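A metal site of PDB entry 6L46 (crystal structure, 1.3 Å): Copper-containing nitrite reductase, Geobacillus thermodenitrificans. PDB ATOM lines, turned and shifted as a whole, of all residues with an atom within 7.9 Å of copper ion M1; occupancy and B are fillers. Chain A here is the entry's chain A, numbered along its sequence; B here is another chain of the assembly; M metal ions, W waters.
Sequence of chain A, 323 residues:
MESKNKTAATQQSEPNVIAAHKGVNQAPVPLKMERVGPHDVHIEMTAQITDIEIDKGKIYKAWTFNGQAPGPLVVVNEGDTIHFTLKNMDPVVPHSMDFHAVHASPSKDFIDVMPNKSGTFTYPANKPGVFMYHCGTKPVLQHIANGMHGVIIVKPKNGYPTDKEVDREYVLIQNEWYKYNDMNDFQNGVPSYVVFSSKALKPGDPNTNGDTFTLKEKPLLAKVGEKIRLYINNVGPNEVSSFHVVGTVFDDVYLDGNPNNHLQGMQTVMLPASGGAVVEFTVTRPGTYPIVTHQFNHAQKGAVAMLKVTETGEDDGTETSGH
A ring nitrogen (NE2) of His 294 of chain B is bound to copper ion M1.
Copper ion M1 is bound by a ring nitrogen (NE2) of His 100 (2.0 Å).
Copper ion M1 is bound by water W2 (2.0 Å).
NE2 of His 134 binds copper ion M1 (2.1 Å).
Water W1 binds copper ion M1, 2.2 Å away.
Copper ion M1 has five donor atoms within binding distance.
N of Asp 98 lies within hydrogen-bond range of O of His 134.
The side-chain amide oxygen (OE1) of Gln 267 of chain B is in hydrogen-bond range of a ring nitrogen (ND1) of His 100 (2.8 Å).
The backbone carbonyl oxygen (O) of Met 132 is in hydrogen-bond range of the backbone NH (N) of His 100.
A ring nitrogen (ND1) of His 244 of chain B is in hydrogen-bond range of the side-chain hydroxyl of Thr 268 of chain B, 3.3 Å away.
O of His 244 of chain B lies within hydrogen-bond range of N of Val 292 of chain B, 2.9 Å away.
A ring nitrogen (ND1) of His 244 of chain B sits at hydrogen-bond distance from the backbone carbonyl oxygen (O) of Gln 267 of chain B, 2.7 Å away.
OD2 of Asp 98 touches copper ion M1, 3.8 Å away.
His 244 of chain B touches copper ion M1.
Of the 23 residues printed, 5 come within 4 Å of copper ion M1.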
ATOM      1  N   ASP A  98      10.871  23.266  24.854  1.00  0.00           N
ATOM      2  CA  ASP A  98      10.769  22.678  26.177  1.00  0.00           C
ATOM      3  C   ASP A  98      10.794  23.854  27.136  1.00  0.00           C
ATOM      4  O   ASP A  98      11.793  24.579  27.211  1.00  0.00           O
ATOM      5  CB  ASP A  98      11.977  21.774  26.372  1.00  0.00           C
ATOM      6  CG  ASP A  98      12.108  21.224  27.769  1.00  0.00           C
ATOM      7  OD1 ASP A  98      11.581  21.812  28.714  1.00  0.00           O
ATOM      8  OD2 ASP A  98      12.808  20.203  27.910  1.00  0.00           O
ATOM      9  N   PHE A  99       9.701  24.069  27.849  1.00  0.00           N
ATOM     10  CA  PHE A  99       9.669  25.058  28.910  1.00  0.00           C
ATOM     11  C   PHE A  99       9.860  24.343  30.236  1.00  0.00           C
ATOM     12  O   PHE A  99       9.053  23.478  30.590  1.00  0.00           O
ATOM     13  CB  PHE A  99       8.315  25.761  28.989  1.00  0.00           C
ATOM     14  CG  PHE A  99       8.020  26.702  27.849  1.00  0.00           C
ATOM     15  CD1 PHE A  99       8.590  27.979  27.816  1.00  0.00           C
ATOM     16  CD2 PHE A  99       7.106  26.352  26.880  1.00  0.00           C
ATOM     17  CE1 PHE A  99       8.270  28.865  26.792  1.00  0.00           C
ATOM     18  CE2 PHE A  99       6.780  27.239  25.863  1.00  0.00           C
ATOM     19  CZ  PHE A  99       7.366  28.489  25.811  1.00  0.00           C
ATOM     20  N   HIS A 100      10.893  24.735  30.999  1.00  0.00           N
ATOM     21  CA  HIS A 100      11.053  24.112  32.315  1.00  0.00           C
ATOM     22  C   HIS A 100       9.934  24.483  33.262  1.00  0.00           C
ATOM     23  O   HIS A 100       9.784  23.872  34.318  1.00  0.00           O
ATOM     24  CB  HIS A 100      12.356  24.509  32.958  1.00  0.00           C
ATOM     25  CG  HIS A 100      13.541  23.797  32.394  1.00  0.00           C
ATOM     26  ND1 HIS A 100      14.748  23.807  33.049  1.00  0.00           N
ATOM     27  CD2 HIS A 100      13.708  23.032  31.284  1.00  0.00           C
ATOM     28  CE1 HIS A 100      15.620  23.091  32.367  1.00  0.00           C
ATOM     29  NE2 HIS A 100      15.018  22.598  31.297  1.00  0.00           N
ATOM     30  N   PHE A 110       6.663  18.350  23.641  1.00  0.00           N
ATOM     31  CA  PHE A 110       7.918  19.012  23.329  1.00  0.00           C
ATOM     32  C   PHE A 110       8.496  18.442  22.034  1.00  0.00           C
ATOM     33  O   PHE A 110       9.707  18.372  21.880  1.00  0.00           O
ATOM     34  CB  PHE A 110       8.947  18.866  24.441  1.00  0.00           C
ATOM     35  CG  PHE A 110       8.570  19.464  25.784  1.00  0.00           C
ATOM     36  CD1 PHE A 110       7.559  20.378  25.946  1.00  0.00           C
ATOM     37  CD2 PHE A 110       9.340  19.121  26.889  1.00  0.00           C
ATOM     38  CE1 PHE A 110       7.295  20.938  27.209  1.00  0.00           C
ATOM     39  CE2 PHE A 110       9.078  19.671  28.142  1.00  0.00           C
ATOM     40  CZ  PHE A 110       8.074  20.583  28.297  1.00  0.00           C
ATOM     41  N   MET A 132      14.293  28.041  32.770  1.00  0.00           N
ATOM     42  CA  MET A 132      14.848  27.964  31.449  1.00  0.00           C
ATOM     43  C   MET A 132      13.814  27.421  30.480  1.00  0.00           C
ATOM     44  O   MET A 132      13.010  26.550  30.811  1.00  0.00           O
ATOM     45  CB  MET A 132      16.063  27.041  31.457  1.00  0.00           C
ATOM     46  CG  MET A 132      16.680  26.859  30.094  1.00  0.00           C
ATOM     47  SD  MET A 132      18.216  25.952  30.282  1.00  0.00           S
ATOM     48  CE  MET A 132      18.754  25.800  28.568  1.00  0.00           C
ATOM     49  N   TYR A 133      13.873  27.908  29.253  1.00  0.00           N
ATOM     50  CA  TYR A 133      13.269  27.204  28.145  1.00  0.00           C
ATOM     51  C   TYR A 133      14.345  26.952  27.114  1.00  0.00           C
ATOM     52  O   TYR A 133      15.363  27.633  27.062  1.00  0.00           O
ATOM     53  CB  TYR A 133      12.059  27.941  27.565  1.00  0.00           C
ATOM     54  CG  TYR A 133      12.302  29.224  26.779  1.00  0.00           C
ATOM     55  CD1 TYR A 133      12.889  29.200  25.532  1.00  0.00           C
ATOM     56  CD2 TYR A 133      11.863  30.439  27.281  1.00  0.00           C
ATOM     57  CE1 TYR A 133      13.063  30.366  24.791  1.00  0.00           C
ATOM     58  CE2 TYR A 133      12.004  31.620  26.548  1.00  0.00           C
ATOM     59  CZ  TYR A 133      12.613  31.561  25.302  1.00  0.00           C
ATOM     60  OH  TYR A 133      12.791  32.664  24.524  1.00  0.00           O
ATOM     61  N   HIS A 134      14.107  25.953  26.274  1.00  0.00           N
ATOM     62  CA  HIS A 134      15.112  25.674  25.266  1.00  0.00           C
ATOM     63  C   HIS A 134      14.528  24.748  24.229  1.00  0.00           C
ATOM     64  O   HIS A 134      13.528  24.072  24.466  1.00  0.00           O
ATOM     65  CB  HIS A 134      16.360  25.075  25.906  1.00  0.00           C
ATOM     66  CG  HIS A 134      16.126  23.798  26.658  1.00  0.00           C
ATOM     67  ND1 HIS A 134      16.088  22.571  26.050  1.00  0.00           N
ATOM     68  CD2 HIS A 134      15.941  23.562  27.986  1.00  0.00           C
ATOM     69  CE1 HIS A 134      15.896  21.625  26.961  1.00  0.00           C
ATOM     70  NE2 HIS A 134      15.808  22.204  28.149  1.00  0.00           N
ATOM     71  N   CYS A 135      15.188  24.688  23.090  1.00  0.00           N
ATOM     72  CA  CYS A 135      14.845  23.683  22.107  1.00  0.00           C
ATOM     73  C   CYS A 135      15.158  22.303  22.664  1.00  0.00           C
ATOM     74  O   CYS A 135      16.175  22.109  23.325  1.00  0.00           O
ATOM     75  CB  CYS A 135      15.632  23.956  20.843  1.00  0.00           C
ATOM     76  SG  CYS A 135      15.295  22.779  19.555  1.00  0.00           S
ATOM     77  N   GLY A 136      14.290  21.345  22.376  1.00  0.00           N
ATOM     78  CA  GLY A 136      14.397  20.002  22.879  1.00  0.00           C
ATOM     79  C   GLY A 136      14.645  18.967  21.812  1.00  0.00           C
ATOM     80  O   GLY A 136      14.388  17.793  22.023  1.00  0.00           O
ATOM     81  N   VAL A 140      20.081  17.605  21.867  1.00  0.00           N
ATOM     82  CA  VAL A 140      19.666  18.804  22.580  1.00  0.00           C
ATOM     83  C   VAL A 140      20.853  19.716  22.821  1.00  0.00           C
ATOM     84  O   VAL A 140      20.743  20.933  22.710  1.00  0.00           O
ATOM     85  CB  VAL A 140      18.945  18.413  23.879  1.00  0.00           C
ATOM     86  CG1 VAL A 140      18.634  19.664  24.694  1.00  0.00           C
ATOM     87  CG2 VAL A 140      17.667  17.671  23.511  1.00  0.00           C
ATOM     88  N   ILE A 144      20.744  23.692  22.019  1.00  0.00           N
ATOM     89  CA  ILE A 144      20.983  24.694  23.043  1.00  0.00           C
ATOM     90  C   ILE A 144      22.242  25.484  22.734  1.00  0.00           C
ATOM     91  O   ILE A 144      22.243  26.718  22.754  1.00  0.00           O
ATOM     92  CB  ILE A 144      21.071  24.052  24.435  1.00  0.00           C
ATOM     93  CG1 ILE A 144      19.741  23.379  24.803  1.00  0.00           C
ATOM     94  CG2 ILE A 144      21.431  25.143  25.456  1.00  0.00           C
ATOM     95  CD1 ILE A 144      19.793  22.672  26.162  1.00  0.00           C
ATOM     96  N   ALA A 273      23.423  24.405  35.727  1.00  0.00           N
ATOM     97  CA  ALA A 273      23.003  24.656  34.360  1.00  0.00           C
ATOM     98  C   ALA A 273      21.491  24.497  34.335  1.00  0.00           C
ATOM     99  O   ALA A 273      20.967  23.477  34.801  1.00  0.00           O
ATOM    100  CB  ALA A 273      23.648  23.661  33.413  1.00  0.00           C
ATOM    101  N   SER A 274      20.813  25.514  33.807  1.00  0.00           N
ATOM    102  CA  SER A 274      19.372  25.752  33.784  1.00  0.00           C
ATOM    103  C   SER A 274      18.852  26.327  35.078  1.00  0.00           C
ATOM    104  O   SER A 274      17.648  26.547  35.189  1.00  0.00           O
ATOM    105  CB  SER A 274      18.505  24.552  33.399  1.00  0.00           C
ATOM    106  OG  SER A 274      18.420  23.572  34.421  1.00  0.00           O
ATOM    107  N   HIS B 244      17.786  17.267  36.449  1.00  0.00           N
ATOM    108  CA  HIS B 244      16.526  17.815  35.963  1.00  0.00           C
ATOM    109  C   HIS B 244      15.701  16.695  35.346  1.00  0.00           C
ATOM    110  O   HIS B 244      16.245  15.886  34.596  1.00  0.00           O
ATOM    111  CB  HIS B 244      16.840  18.850  34.881  1.00  0.00           C
ATOM    112  CG  HIS B 244      15.631  19.404  34.204  1.00  0.00           C
ATOM    113  ND1 HIS B 244      14.796  20.312  34.806  1.00  0.00           N
ATOM    114  CD2 HIS B 244      15.111  19.163  32.970  1.00  0.00           C
ATOM    115  CE1 HIS B 244      13.810  20.604  33.997  1.00  0.00           C
ATOM    116  NE2 HIS B 244      13.975  19.925  32.879  1.00  0.00           N
ATOM    117  N   VAL B 245      14.402  16.697  35.614  1.00  0.00           N
ATOM    118  CA  VAL B 245      13.474  15.809  34.928  1.00  0.00           C
ATOM    119  C   VAL B 245      12.674  16.652  33.944  1.00  0.00           C
ATOM    120  O   VAL B 245      12.017  17.624  34.321  1.00  0.00           O
ATOM    121  CB  VAL B 245      12.577  15.044  35.906  1.00  0.00           C
ATOM    122  CG1 VAL B 245      11.622  14.127  35.129  1.00  0.00           C
ATOM    123  CG2 VAL B 245      13.413  14.224  36.862  1.00  0.00           C
ATOM    124  N   VAL B 246      12.761  16.286  32.676  1.00  0.00           N
ATOM    125  CA  VAL B 246      12.074  17.015  31.630  1.00  0.00           C
ATOM    126  C   VAL B 246      10.577  16.810  31.770  1.00  0.00           C
ATOM    127  O   VAL B 246      10.107  15.702  32.000  1.00  0.00           O
ATOM    128  CB  VAL B 246      12.574  16.481  30.279  1.00  0.00           C
ATOM    129  CG1 VAL B 246      11.866  17.180  29.135  1.00  0.00           C
ATOM    130  CG2 VAL B 246      14.087  16.668  30.172  1.00  0.00           C
ATOM    131  N   GLY B 247       9.823  17.883  31.593  1.00  0.00           N
ATOM    132  CA  GLY B 247       8.382  17.808  31.588  1.00  0.00           C
ATOM    133  C   GLY B 247       7.749  17.916  32.953  1.00  0.00           C
ATOM    134  O   GLY B 247       6.525  17.816  33.063  1.00  0.00           O
ATOM    135  N   GLN B 267      13.344  23.577  39.416  1.00  0.00           N
ATOM    136  CA  GLN B 267      13.421  22.973  38.096  1.00  0.00           C
ATOM    137  C   GLN B 267      14.579  21.995  38.034  1.00  0.00           C
ATOM    138  O   GLN B 267      14.475  20.980  37.356  1.00  0.00           O
ATOM    139  CB  GLN B 267      13.572  24.047  37.030  1.00  0.00           C
ATOM    140  CG  GLN B 267      14.911  24.757  36.957  1.00  0.00           C
ATOM    141  CD  GLN B 267      14.779  25.991  36.117  1.00  0.00           C
ATOM    142  OE1 GLN B 267      14.526  25.915  34.905  1.00  0.00           O
ATOM    143  NE2 GLN B 267      14.926  27.151  36.748  1.00  0.00           N
ATOM    144  N   THR B 268      15.671  22.296  38.721  1.00  0.00           N
ATOM    145  CA  THR B 268      16.928  21.596  38.576  1.00  0.00           C
ATOM    146  C   THR B 268      17.611  21.639  39.931  1.00  0.00           C
ATOM    147  O   THR B 268      17.543  22.650  40.628  1.00  0.00           O
ATOM    148  CB  THR B 268      17.767  22.320  37.524  1.00  0.00           C
ATOM    149  OG1 THR B 268      17.058  22.162  36.286  1.00  0.00           O
ATOM    150  CG2 THR B 268      19.186  21.726  37.399  1.00  0.00           C
ATOM    151  N   VAL B 292      17.923  14.075  33.117  1.00  0.00           N
ATOM    152  CA  VAL B 292      19.227  14.513  32.637  1.00  0.00           C
ATOM    153  C   VAL B 292      20.018  15.146  33.760  1.00  0.00           C
ATOM    154  O   VAL B 292      19.473  15.622  34.756  1.00  0.00           O
ATOM    155  CB  VAL B 292      19.081  15.523  31.470  1.00  0.00           C
ATOM    156  CG1 VAL B 292      18.215  14.931  30.350  1.00  0.00           C
ATOM    157  CG2 VAL B 292      18.512  16.861  31.917  1.00  0.00           C
ATOM    158  N   THR B 293      21.325  15.259  33.528  1.00  0.00           N
ATOM    159  CA  THR B 293      22.038  16.403  34.032  1.00  0.00           C
ATOM    160  C   THR B 293      21.956  17.480  32.952  1.00  0.00           C
ATOM    161  O   THR B 293      22.174  17.216  31.773  1.00  0.00           O
ATOM    162  CB  THR B 293      23.482  16.113  34.422  1.00  0.00           C
ATOM    163  OG1 THR B 293      24.081  17.374  34.746  1.00  0.00           O
ATOM    164  CG2 THR B 293      24.248  15.444  33.303  1.00  0.00           C
ATOM    165  N   HIS B 294      21.588  18.686  33.356  1.00  0.00           N
ATOM    166  CA  HIS B 294      21.384  19.751  32.387  1.00  0.00           C
ATOM    167  C   HIS B 294      22.674  20.414  31.969  1.00  0.00           C
ATOM    168  O   HIS B 294      22.635  21.338  31.163  1.00  0.00           O
ATOM    169  CB  HIS B 294      20.408  20.789  32.935  1.00  0.00           C
ATOM    170  CG  HIS B 294      19.421  21.259  31.928  1.00  0.00           C
ATOM    171  ND1 HIS B 294      19.706  22.146  30.924  1.00  0.00           N
ATOM    172  CD2 HIS B 294      18.123  20.897  31.748  1.00  0.00           C
ATOM    173  CE1 HIS B 294      18.625  22.331  30.175  1.00  0.00           C
ATOM    174  NE2 HIS B 294      17.650  21.577  30.666  1.00  0.00           N
ATOM    175  N   PHE B 296      24.776  19.967  29.492  1.00  0.00           N
ATOM    176  CA  PHE B 296      24.366  19.164  28.356  1.00  0.00           C
ATOM    177  C   PHE B 296      25.524  18.474  27.648  1.00  0.00           C
ATOM    178  O   PHE B 296      25.287  17.514  26.913  1.00  0.00           O
ATOM    179  CB  PHE B 296      23.420  19.912  27.408  1.00  0.00           C
ATOM    180  CG  PHE B 296      22.019  19.394  27.545  1.00  0.00           C
ATOM    181  CD1 PHE B 296      21.633  18.244  26.851  1.00  0.00           C
ATOM    182  CD2 PHE B 296      21.159  19.934  28.477  1.00  0.00           C
ATOM    183  CE1 PHE B 296      20.392  17.676  27.056  1.00  0.00           C
ATOM    184  CE2 PHE B 296      19.917  19.377  28.692  1.00  0.00           C
ATOM    185  CZ  PHE B 296      19.525  18.248  27.973  1.00  0.00           C
HETATM  186 CU    CU M   1      15.828  21.296  30.003  1.00  0.00          CU
HETATM  187 CU    CU M   2      12.841  20.285  31.685  1.00  0.00          CU
HETATM  188  O   HOH W   1      16.288  19.276  29.230  1.00  0.00           O
HETATM  189  O   HOH W   2      14.100  20.238  30.064  1.00  0.00           O
